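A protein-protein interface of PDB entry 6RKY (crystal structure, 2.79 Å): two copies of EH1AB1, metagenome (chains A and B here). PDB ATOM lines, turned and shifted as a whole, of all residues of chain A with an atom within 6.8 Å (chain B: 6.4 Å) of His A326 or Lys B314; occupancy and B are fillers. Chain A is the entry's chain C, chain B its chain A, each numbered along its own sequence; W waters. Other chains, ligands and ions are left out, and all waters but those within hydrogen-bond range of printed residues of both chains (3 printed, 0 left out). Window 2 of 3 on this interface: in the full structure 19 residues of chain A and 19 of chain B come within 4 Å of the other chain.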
ATOM      1  N   ARG A 168      -3.898 -25.251  -2.055  1.00  0.00           N
ATOM      2  CA  ARG A 168      -4.251 -24.370  -3.197  1.00  0.00           C
ATOM      3  C   ARG A 168      -2.977 -23.737  -3.759  1.00  0.00           C
ATOM      4  O   ARG A 168      -2.873 -22.501  -3.829  1.00  0.00           O
ATOM      5  CB  ARG A 168      -5.318 -23.360  -2.762  1.00  0.00           C
ATOM      6  CG  ARG A 168      -6.664 -24.017  -2.512  1.00  0.00           C
ATOM      7  CD  ARG A 168      -7.717 -23.011  -2.124  1.00  0.00           C
ATOM      8  NE  ARG A 168      -7.269 -22.249  -0.969  1.00  0.00           N
ATOM      9  CZ  ARG A 168      -7.715 -21.051  -0.612  1.00  0.00           C
ATOM     10  NH1 ARG A 168      -8.646 -20.426  -1.319  1.00  0.00           N
ATOM     11  NH2 ARG A 168      -7.205 -20.482   0.464  1.00  0.00           N
ATOM     12  N   ALA A 197      -2.198 -27.902  -7.789  1.00  0.00           N
ATOM     13  CA  ALA A 197      -3.664 -28.045  -7.679  1.00  0.00           C
ATOM     14  C   ALA A 197      -4.325 -27.386  -8.902  1.00  0.00           C
ATOM     15  O   ALA A 197      -5.590 -27.492  -9.038  1.00  0.00           O
ATOM     16  CB  ALA A 197      -4.110 -27.427  -6.380  1.00  0.00           C
ATOM     17  N   PHE A 198      -3.509 -26.726  -9.738  1.00  0.00           N
ATOM     18  CA  PHE A 198      -3.958 -25.991 -10.943  1.00  0.00           C
ATOM     19  C   PHE A 198      -2.748 -25.620 -11.796  1.00  0.00           C
ATOM     20  O   PHE A 198      -1.660 -25.306 -11.218  1.00  0.00           O
ATOM     21  CB  PHE A 198      -4.734 -24.756 -10.520  1.00  0.00           C
ATOM     22  CG  PHE A 198      -5.519 -24.116 -11.630  1.00  0.00           C
ATOM     23  CD1 PHE A 198      -4.915 -23.241 -12.519  1.00  0.00           C
ATOM     24  CD2 PHE A 198      -6.881 -24.356 -11.763  1.00  0.00           C
ATOM     25  CE1 PHE A 198      -5.645 -22.644 -13.528  1.00  0.00           C
ATOM     26  CE2 PHE A 198      -7.610 -23.734 -12.767  1.00  0.00           C
ATOM     27  CZ  PHE A 198      -6.990 -22.876 -13.640  1.00  0.00           C
ATOM     28  N   PRO A 261      -6.396 -29.536 -12.800  1.00  0.00           N
ATOM     29  CA  PRO A 261      -7.235 -28.680 -13.635  1.00  0.00           C
ATOM     30  C   PRO A 261      -6.366 -27.615 -14.313  1.00  0.00           C
ATOM     31  O   PRO A 261      -5.421 -27.170 -13.711  1.00  0.00           O
ATOM     32  CB  PRO A 261      -8.238 -28.070 -12.655  1.00  0.00           C
ATOM     33  CG  PRO A 261      -8.325 -29.113 -11.548  1.00  0.00           C
ATOM     34  CD  PRO A 261      -6.948 -29.743 -11.457  1.00  0.00           C
ATOM     35  N   LYS A 289     -10.861 -31.143 -15.625  1.00  0.00           N
ATOM     36  CA  LYS A 289     -11.537 -29.816 -15.693  1.00  0.00           C
ATOM     37  C   LYS A 289     -10.560 -28.862 -16.387  1.00  0.00           C
ATOM     38  O   LYS A 289      -9.372 -28.863 -16.006  1.00  0.00           O
ATOM     39  CB  LYS A 289     -12.003 -29.363 -14.302  1.00  0.00           C
ATOM     40  CG  LYS A 289     -11.940 -27.868 -14.003  1.00  0.00           C
ATOM     41  CD  LYS A 289     -13.055 -27.027 -14.570  1.00  0.00           C
ATOM     42  CE  LYS A 289     -12.899 -25.552 -14.248  1.00  0.00           C
ATOM     43  NZ  LYS A 289     -12.668 -25.303 -12.797  1.00  0.00           N
ATOM     44  N   ALA A 321      -9.000 -14.194 -13.121  1.00  0.00           N
ATOM     45  CA  ALA A 321     -10.420 -14.443 -12.786  1.00  0.00           C
ATOM     46  C   ALA A 321     -10.725 -15.943 -12.712  1.00  0.00           C
ATOM     47  O   ALA A 321     -11.328 -16.373 -11.726  1.00  0.00           O
ATOM     48  CB  ALA A 321     -11.282 -13.755 -13.813  1.00  0.00           C
ATOM     49  N   VAL A 322     -10.344 -16.716 -13.727  1.00  0.00           N
ATOM     50  CA  VAL A 322     -10.542 -18.198 -13.771  1.00  0.00           C
ATOM     51  C   VAL A 322      -9.871 -18.852 -12.554  1.00  0.00           C
ATOM     52  O   VAL A 322     -10.496 -19.754 -11.971  1.00  0.00           O
ATOM     53  CB  VAL A 322     -10.022 -18.809 -15.075  1.00  0.00           C
ATOM     54  CG1 VAL A 322      -9.895 -20.333 -14.998  1.00  0.00           C
ATOM     55  CG2 VAL A 322     -10.907 -18.411 -16.235  1.00  0.00           C
ATOM     56  N   MET A 323      -8.650 -18.430 -12.192  1.00  0.00           N
ATOM     57  CA  MET A 323      -7.869 -19.054 -11.085  1.00  0.00           C
ATOM     58  C   MET A 323      -8.494 -18.685  -9.742  1.00  0.00           C
ATOM     59  O   MET A 323      -8.478 -19.532  -8.852  1.00  0.00           O
ATOM     60  CB  MET A 323      -6.405 -18.601 -11.090  1.00  0.00           C
ATOM     61  CG  MET A 323      -5.531 -19.396 -10.135  1.00  0.00           C
ATOM     62  SD  MET A 323      -3.769 -18.998 -10.265  1.00  0.00           S
ATOM     63  CE  MET A 323      -3.787 -17.271  -9.792  1.00  0.00           C
ATOM     64  N   GLY A 324      -8.984 -17.451  -9.602  1.00  0.00           N
ATOM     65  CA  GLY A 324      -9.728 -16.966  -8.418  1.00  0.00           C
ATOM     66  C   GLY A 324     -11.016 -17.743  -8.204  1.00  0.00           C
ATOM     67  O   GLY A 324     -11.320 -18.077  -7.028  1.00  0.00           O
ATOM     68  N   ALA A 325     -11.741 -18.026  -9.300  1.00  0.00           N
ATOM     69  CA  ALA A 325     -12.984 -18.830  -9.302  1.00  0.00           C
ATOM     70  C   ALA A 325     -12.679 -20.252  -8.808  1.00  0.00           C
ATOM     71  O   ALA A 325     -13.490 -20.765  -8.010  1.00  0.00           O
ATOM     72  CB  ALA A 325     -13.614 -18.838 -10.662  1.00  0.00           C
ATOM     73  N   HIS A 326     -11.549 -20.848  -9.215  1.00  0.00           N
ATOM     74  CA  HIS A 326     -11.179 -22.249  -8.864  1.00  0.00           C
ATOM     75  C   HIS A 326     -10.868 -22.367  -7.372  1.00  0.00           C
ATOM     76  O   HIS A 326     -11.287 -23.371  -6.765  1.00  0.00           O
ATOM     77  CB  HIS A 326     -10.000 -22.778  -9.677  1.00  0.00           C
ATOM     78  CG  HIS A 326      -9.699 -24.209  -9.380  1.00  0.00           C
ATOM     79  ND1 HIS A 326     -10.387 -25.247  -9.979  1.00  0.00           N
ATOM     80  CD2 HIS A 326      -8.801 -24.777  -8.549  1.00  0.00           C
ATOM     81  CE1 HIS A 326      -9.907 -26.398  -9.540  1.00  0.00           C
ATOM     82  NE2 HIS A 326      -8.932 -26.136  -8.655  1.00  0.00           N
ATOM     83  N   PHE A 327     -10.124 -21.398  -6.837  1.00  0.00           N
ATOM     84  CA  PHE A 327      -9.597 -21.368  -5.443  1.00  0.00           C
ATOM     85  C   PHE A 327     -10.568 -20.635  -4.508  1.00  0.00           C
ATOM     86  O   PHE A 327     -10.291 -20.571  -3.297  1.00  0.00           O
ATOM     87  CB  PHE A 327      -8.221 -20.696  -5.398  1.00  0.00           C
ATOM     88  CG  PHE A 327      -7.105 -21.524  -5.953  1.00  0.00           C
ATOM     89  CD1 PHE A 327      -7.152 -22.917  -5.909  1.00  0.00           C
ATOM     90  CD2 PHE A 327      -5.988 -20.917  -6.489  1.00  0.00           C
ATOM     91  CE1 PHE A 327      -6.111 -23.681  -6.411  1.00  0.00           C
ATOM     92  CE2 PHE A 327      -4.953 -21.686  -7.004  1.00  0.00           C
ATOM     93  CZ  PHE A 327      -5.020 -23.065  -6.970  1.00  0.00           C
ATOM     94  N   GLY A 328     -11.650 -20.073  -5.056  1.00  0.00           N
ATOM     95  CA  GLY A 328     -12.740 -19.452  -4.277  1.00  0.00           C
ATOM     96  C   GLY A 328     -12.287 -18.203  -3.556  1.00  0.00           C
ATOM     97  O   GLY A 328     -12.803 -17.950  -2.454  1.00  0.00           O
ATOM     98  N   THR A 329     -11.387 -17.433  -4.170  1.00  0.00           N
ATOM     99  CA  THR A 329     -10.745 -16.241  -3.551  1.00  0.00           C
ATOM    100  C   THR A 329     -11.731 -15.065  -3.587  1.00  0.00           C
ATOM    101  O   THR A 329     -12.746 -15.133  -4.287  1.00  0.00           O
ATOM    102  CB  THR A 329      -9.424 -15.881  -4.247  1.00  0.00           C
ATOM    103  OG1 THR A 329      -9.728 -15.306  -5.518  1.00  0.00           O
ATOM    104  CG2 THR A 329      -8.496 -17.061  -4.440  1.00  0.00           C
ATOM    105  OXT THR A 329     -11.546 -14.030  -2.934  1.00  0.00           O
ATOM    106  N   ARG B 119     -26.201 -14.098  -8.105  1.00  0.00           N
ATOM    107  CA  ARG B 119     -24.775 -14.454  -7.961  1.00  0.00           C
ATOM    108  C   ARG B 119     -24.006 -13.991  -9.198  1.00  0.00           C
ATOM    109  O   ARG B 119     -22.942 -13.385  -9.007  1.00  0.00           O
ATOM    110  CB  ARG B 119     -24.600 -15.946  -7.686  1.00  0.00           C
ATOM    111  CG  ARG B 119     -23.203 -16.259  -7.173  1.00  0.00           C
ATOM    112  CD  ARG B 119     -23.004 -17.731  -6.908  1.00  0.00           C
ATOM    113  NE  ARG B 119     -21.620 -18.001  -6.556  1.00  0.00           N
ATOM    114  CZ  ARG B 119     -21.161 -18.107  -5.317  1.00  0.00           C
ATOM    115  NH1 ARG B 119     -21.978 -17.976  -4.287  1.00  0.00           N
ATOM    116  NH2 ARG B 119     -19.879 -18.362  -5.113  1.00  0.00           N
ATOM    117  N   TYR B 295     -16.717 -29.102 -17.362  1.00  0.00           N
ATOM    118  CA  TYR B 295     -16.810 -29.550 -15.963  1.00  0.00           C
ATOM    119  C   TYR B 295     -17.101 -31.036 -16.012  1.00  0.00           C
ATOM    120  O   TYR B 295     -18.253 -31.435 -16.082  1.00  0.00           O
ATOM    121  CB  TYR B 295     -17.844 -28.738 -15.189  1.00  0.00           C
ATOM    122  CG  TYR B 295     -17.314 -27.432 -14.670  1.00  0.00           C
ATOM    123  CD1 TYR B 295     -17.202 -26.325 -15.503  1.00  0.00           C
ATOM    124  CD2 TYR B 295     -16.939 -27.288 -13.348  1.00  0.00           C
ATOM    125  CE1 TYR B 295     -16.739 -25.106 -15.026  1.00  0.00           C
ATOM    126  CE2 TYR B 295     -16.507 -26.067 -12.846  1.00  0.00           C
ATOM    127  CZ  TYR B 295     -16.391 -24.975 -13.694  1.00  0.00           C
ATOM    128  OH  TYR B 295     -15.905 -23.780 -13.232  1.00  0.00           O
ATOM    129  N   LEU B 309     -24.883 -29.137  -5.258  1.00  0.00           N
ATOM    130  CA  LEU B 309     -23.678 -29.279  -6.125  1.00  0.00           C
ATOM    131  C   LEU B 309     -22.800 -28.018  -6.062  1.00  0.00           C
ATOM    132  O   LEU B 309     -23.085 -27.040  -6.792  1.00  0.00           O
ATOM    133  CB  LEU B 309     -24.148 -29.567  -7.556  1.00  0.00           C
ATOM    134  CG  LEU B 309     -25.015 -30.818  -7.719  1.00  0.00           C
ATOM    135  CD1 LEU B 309     -25.409 -31.043  -9.172  1.00  0.00           C
ATOM    136  CD2 LEU B 309     -24.310 -32.040  -7.179  1.00  0.00           C
ATOM    137  N   SER B 310     -21.758 -28.065  -5.222  1.00  0.00           N
ATOM    138  CA  SER B 310     -20.713 -27.017  -5.040  1.00  0.00           C
ATOM    139  C   SER B 310     -20.079 -26.604  -6.375  1.00  0.00           C
ATOM    140  O   SER B 310     -19.765 -25.403  -6.521  1.00  0.00           O
ATOM    141  CB  SER B 310     -19.652 -27.495  -4.091  1.00  0.00           C
ATOM    142  OG  SER B 310     -20.211 -27.699  -2.801  1.00  0.00           O
ATOM    143  N   GLN B 311     -19.874 -27.558  -7.296  1.00  0.00           N
ATOM    144  CA  GLN B 311     -19.280 -27.301  -8.635  1.00  0.00           C
ATOM    145  C   GLN B 311     -20.100 -26.229  -9.366  1.00  0.00           C
ATOM    146  O   GLN B 311     -19.496 -25.447 -10.101  1.00  0.00           O
ATOM    147  CB  GLN B 311     -19.212 -28.578  -9.477  1.00  0.00           C
ATOM    148  CG  GLN B 311     -18.098 -29.545  -9.079  1.00  0.00           C
ATOM    149  CD  GLN B 311     -16.713 -28.958  -9.196  1.00  0.00           C
ATOM    150  OE1 GLN B 311     -16.182 -28.821 -10.299  1.00  0.00           O
ATOM    151  NE2 GLN B 311     -16.117 -28.628  -8.054  1.00  0.00           N
ATOM    152  N   GLY B 312     -21.419 -26.198  -9.169  1.00  0.00           N
ATOM    153  CA  GLY B 312     -22.314 -25.180  -9.748  1.00  0.00           C
ATOM    154  C   GLY B 312     -21.925 -23.762  -9.349  1.00  0.00           C
ATOM    155  O   GLY B 312     -22.032 -22.849 -10.202  1.00  0.00           O
ATOM    156  N   LEU B 313     -21.519 -23.565  -8.094  1.00  0.00           N
ATOM    157  CA  LEU B 313     -21.144 -22.231  -7.562  1.00  0.00           C
ATOM    158  C   LEU B 313     -19.822 -21.790  -8.201  1.00  0.00           C
ATOM    159  O   LEU B 313     -19.726 -20.610  -8.614  1.00  0.00           O
ATOM    160  CB  LEU B 313     -21.042 -22.294  -6.032  1.00  0.00           C
ATOM    161  CG  LEU B 313     -22.382 -22.468  -5.313  1.00  0.00           C
ATOM    162  CD1 LEU B 313     -22.192 -22.838  -3.857  1.00  0.00           C
ATOM    163  CD2 LEU B 313     -23.233 -21.218  -5.434  1.00  0.00           C
ATOM    164  N   LYS B 314     -18.856 -22.706  -8.283  1.00  0.00           N
ATOM    165  CA  LYS B 314     -17.536 -22.496  -8.937  1.00  0.00           C
ATOM    166  C   LYS B 314     -17.745 -22.169 -10.421  1.00  0.00           C
ATOM    167  O   LYS B 314     -17.010 -21.315 -10.940  1.00  0.00           O
ATOM    168  CB  LYS B 314     -16.668 -23.744  -8.777  1.00  0.00           C
ATOM    169  CG  LYS B 314     -16.434 -24.172  -7.339  1.00  0.00           C
ATOM    170  CD  LYS B 314     -15.530 -23.230  -6.576  1.00  0.00           C
ATOM    171  CE  LYS B 314     -14.066 -23.576  -6.727  1.00  0.00           C
ATOM    172  NZ  LYS B 314     -13.728 -24.821  -5.998  1.00  0.00           N
ATOM    173  N   ALA B 315     -18.736 -22.801 -11.058  1.00  0.00           N
ATOM    174  CA  ALA B 315     -19.136 -22.586 -12.470  1.00  0.00           C
ATOM    175  C   ALA B 315     -19.715 -21.178 -12.681  1.00  0.00           C
ATOM    176  O   ALA B 315     -19.288 -20.510 -13.642  1.00  0.00           O
ATOM    177  CB  ALA B 315     -20.118 -23.647 -12.893  1.00  0.00           C
ATOM    178  N   ASN B 316     -20.660 -20.752 -11.833  1.00  0.00           N
ATOM    179  CA  ASN B 316     -21.237 -19.382 -11.847  1.00  0.00           C
ATOM    180  C   ASN B 316     -20.074 -18.399 -11.767  1.00  0.00           C
ATOM    181  O   ASN B 316     -20.063 -17.433 -12.555  1.00  0.00           O
ATOM    182  CB  ASN B 316     -22.178 -19.082 -10.679  1.00  0.00           C
ATOM    183  CG  ASN B 316     -23.395 -19.974 -10.567  1.00  0.00           C
ATOM    184  OD1 ASN B 316     -23.890 -20.189  -9.465  1.00  0.00           O
ATOM    185  ND2 ASN B 316     -23.916 -20.455 -11.680  1.00  0.00           N
ATOM    186  N   ASP B 317     -19.129 -18.635 -10.851  1.00  0.00           N
ATOM    187  CA  ASP B 317     -17.967 -17.721 -10.632  1.00  0.00           C
ATOM    188  C   ASP B 317     -17.063 -17.669 -11.871  1.00  0.00           C
ATOM    189  O   ASP B 317     -16.653 -16.550 -12.260  1.00  0.00           O
ATOM    190  CB  ASP B 317     -17.177 -18.125  -9.402  1.00  0.00           C
ATOM    191  CG  ASP B 317     -18.013 -17.962  -8.147  1.00  0.00           C
ATOM    192  OD1 ASP B 317     -19.063 -17.291  -8.239  1.00  0.00           O
ATOM    193  OD2 ASP B 317     -17.630 -18.538  -7.101  1.00  0.00           O
ATOM    194  N   GLU B 318     -16.800 -18.809 -12.508  1.00  0.00           N
ATOM    195  CA  GLU B 318     -15.984 -18.816 -13.748  1.00  0.00           C
ATOM    196  C   GLU B 318     -16.709 -18.033 -14.848  1.00  0.00           C
ATOM    197  O   GLU B 318     -16.067 -17.196 -15.460  1.00  0.00           O
ATOM    198  CB  GLU B 318     -15.610 -20.218 -14.208  1.00  0.00           C
ATOM    199  CG  GLU B 318     -14.361 -20.176 -15.071  1.00  0.00           C
ATOM    200  CD  GLU B 318     -13.960 -21.466 -15.761  1.00  0.00           C
ATOM    201  OE1 GLU B 318     -13.879 -22.562 -15.086  1.00  0.00           O
ATOM    202  OE2 GLU B 318     -13.695 -21.364 -16.955  1.00  0.00           O
ATOM    203  N   ALA B 319     -18.002 -18.269 -15.052  1.00  0.00           N
ATOM    204  CA  ALA B 319     -18.861 -17.570 -16.045  1.00  0.00           C
ATOM    205  C   ALA B 319     -18.856 -16.064 -15.784  1.00  0.00           C
ATOM    206  O   ALA B 319     -18.565 -15.287 -16.719  1.00  0.00           O
ATOM    207  CB  ALA B 319     -20.268 -18.123 -16.018  1.00  0.00           C
HETATM  208  O   HOH W   1     -13.819 -22.402 -10.977  1.00  0.00           O
HETATM  209  O   HOH W   2     -14.862 -17.175  -5.787  1.00  0.00           O
HETATM  210  O   HOH W   3     -15.008 -19.876  -6.345  1.00  0.00           O
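Water W3 bridges O of Ala A325 (2.4 Å) and OD2 of Asp B317 (3.0 Å).
Water W1 lies within hydrogen-bond range of N of His A326 (3.3 Å), OH of Tyr B295 (3.4 Å), O of Lys B314 (3.4 Å) and O of Ala A325 (3.4 Å).
Water W2 bridges the chain-end carboxylate (O) of Thr A329 and the side-chain carboxylate (OD2) of Asp B317.
No position is printed for both chains.
Of the 6 pairs that touch across the chains among the printed residues, none has its exchanged pair printed and touching as well.
Among the printed residues, merely in contact across the chains: Lys A289 with Tyr B295 (3.6 Å), Ala A325 with Lys B314 (3.1 Å), Ala A325 with Asp B317 (3.8 Å) and Ala A325 with Glu B318 (3.7 Å).
The backbone carbonyl oxygen of His A326 lies close to the side-chain amino group of Lys B314, 2.9 Å away.
The side-chain carboxylate of Glu B318 lies within salt-bridge range of the side-chain amino group of Lys A289 (3.8 Å).
Of chain A, only Ala A325 and His A326 come within 4 Å of Lys B314.
Of the printed residues of chain A, Glu B318 touches Lys A289 and Ala A325.
Of the printed residues of chain A, Tyr B295 touches Lys A289.
Of the printed residues of chain B, Lys A289 touches Tyr B295 (3.6 Å) and Glu B318 (3.3 Å).
Of the printed residues of chain A, Asp B317 touches Ala A325 (3.8 Å).
Printed residues of chain B within 4 Å of Ala A325: Lys B314 (3.1 Å), Asp B317 (3.8 Å) and Glu B318 (3.7 Å).
Phe A198 touches none of the printed residues of chain B.
Pro A261 touches none of the printed residues of chain B.
The nearest residue of chain B that does not touch His A326 is Asp B317 (6.3 Å).
The nearest residue of chain A that does not touch Lys B314 is Phe A327 (4.5 Å).
The side-chain carboxylate of Glu B318 sits at hydrogen-bond distance from the side-chain hydroxyl of Tyr B295, at 3.0 Å.
NH2 of Arg B119 is in salt-bridge range of OD2 of Asp B317.
Hydrophobic or aromatic side chains of chain A that line the printed part of chain B: Ala A325.
Of the 13 printed residues of chain B, 4 touch a printed residue of chain A.
Hydrophobic or aromatic side chains of chain B that line the printed part of chain A: Tyr B295.
Among the printed residues, 6 pairs touch across the chains.
Among the printed residues, Asp or Glu carboxylates within 4 Å of a Lys or Arg side-chain nitrogen of the other chain: Lys A289 with Glu B318.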
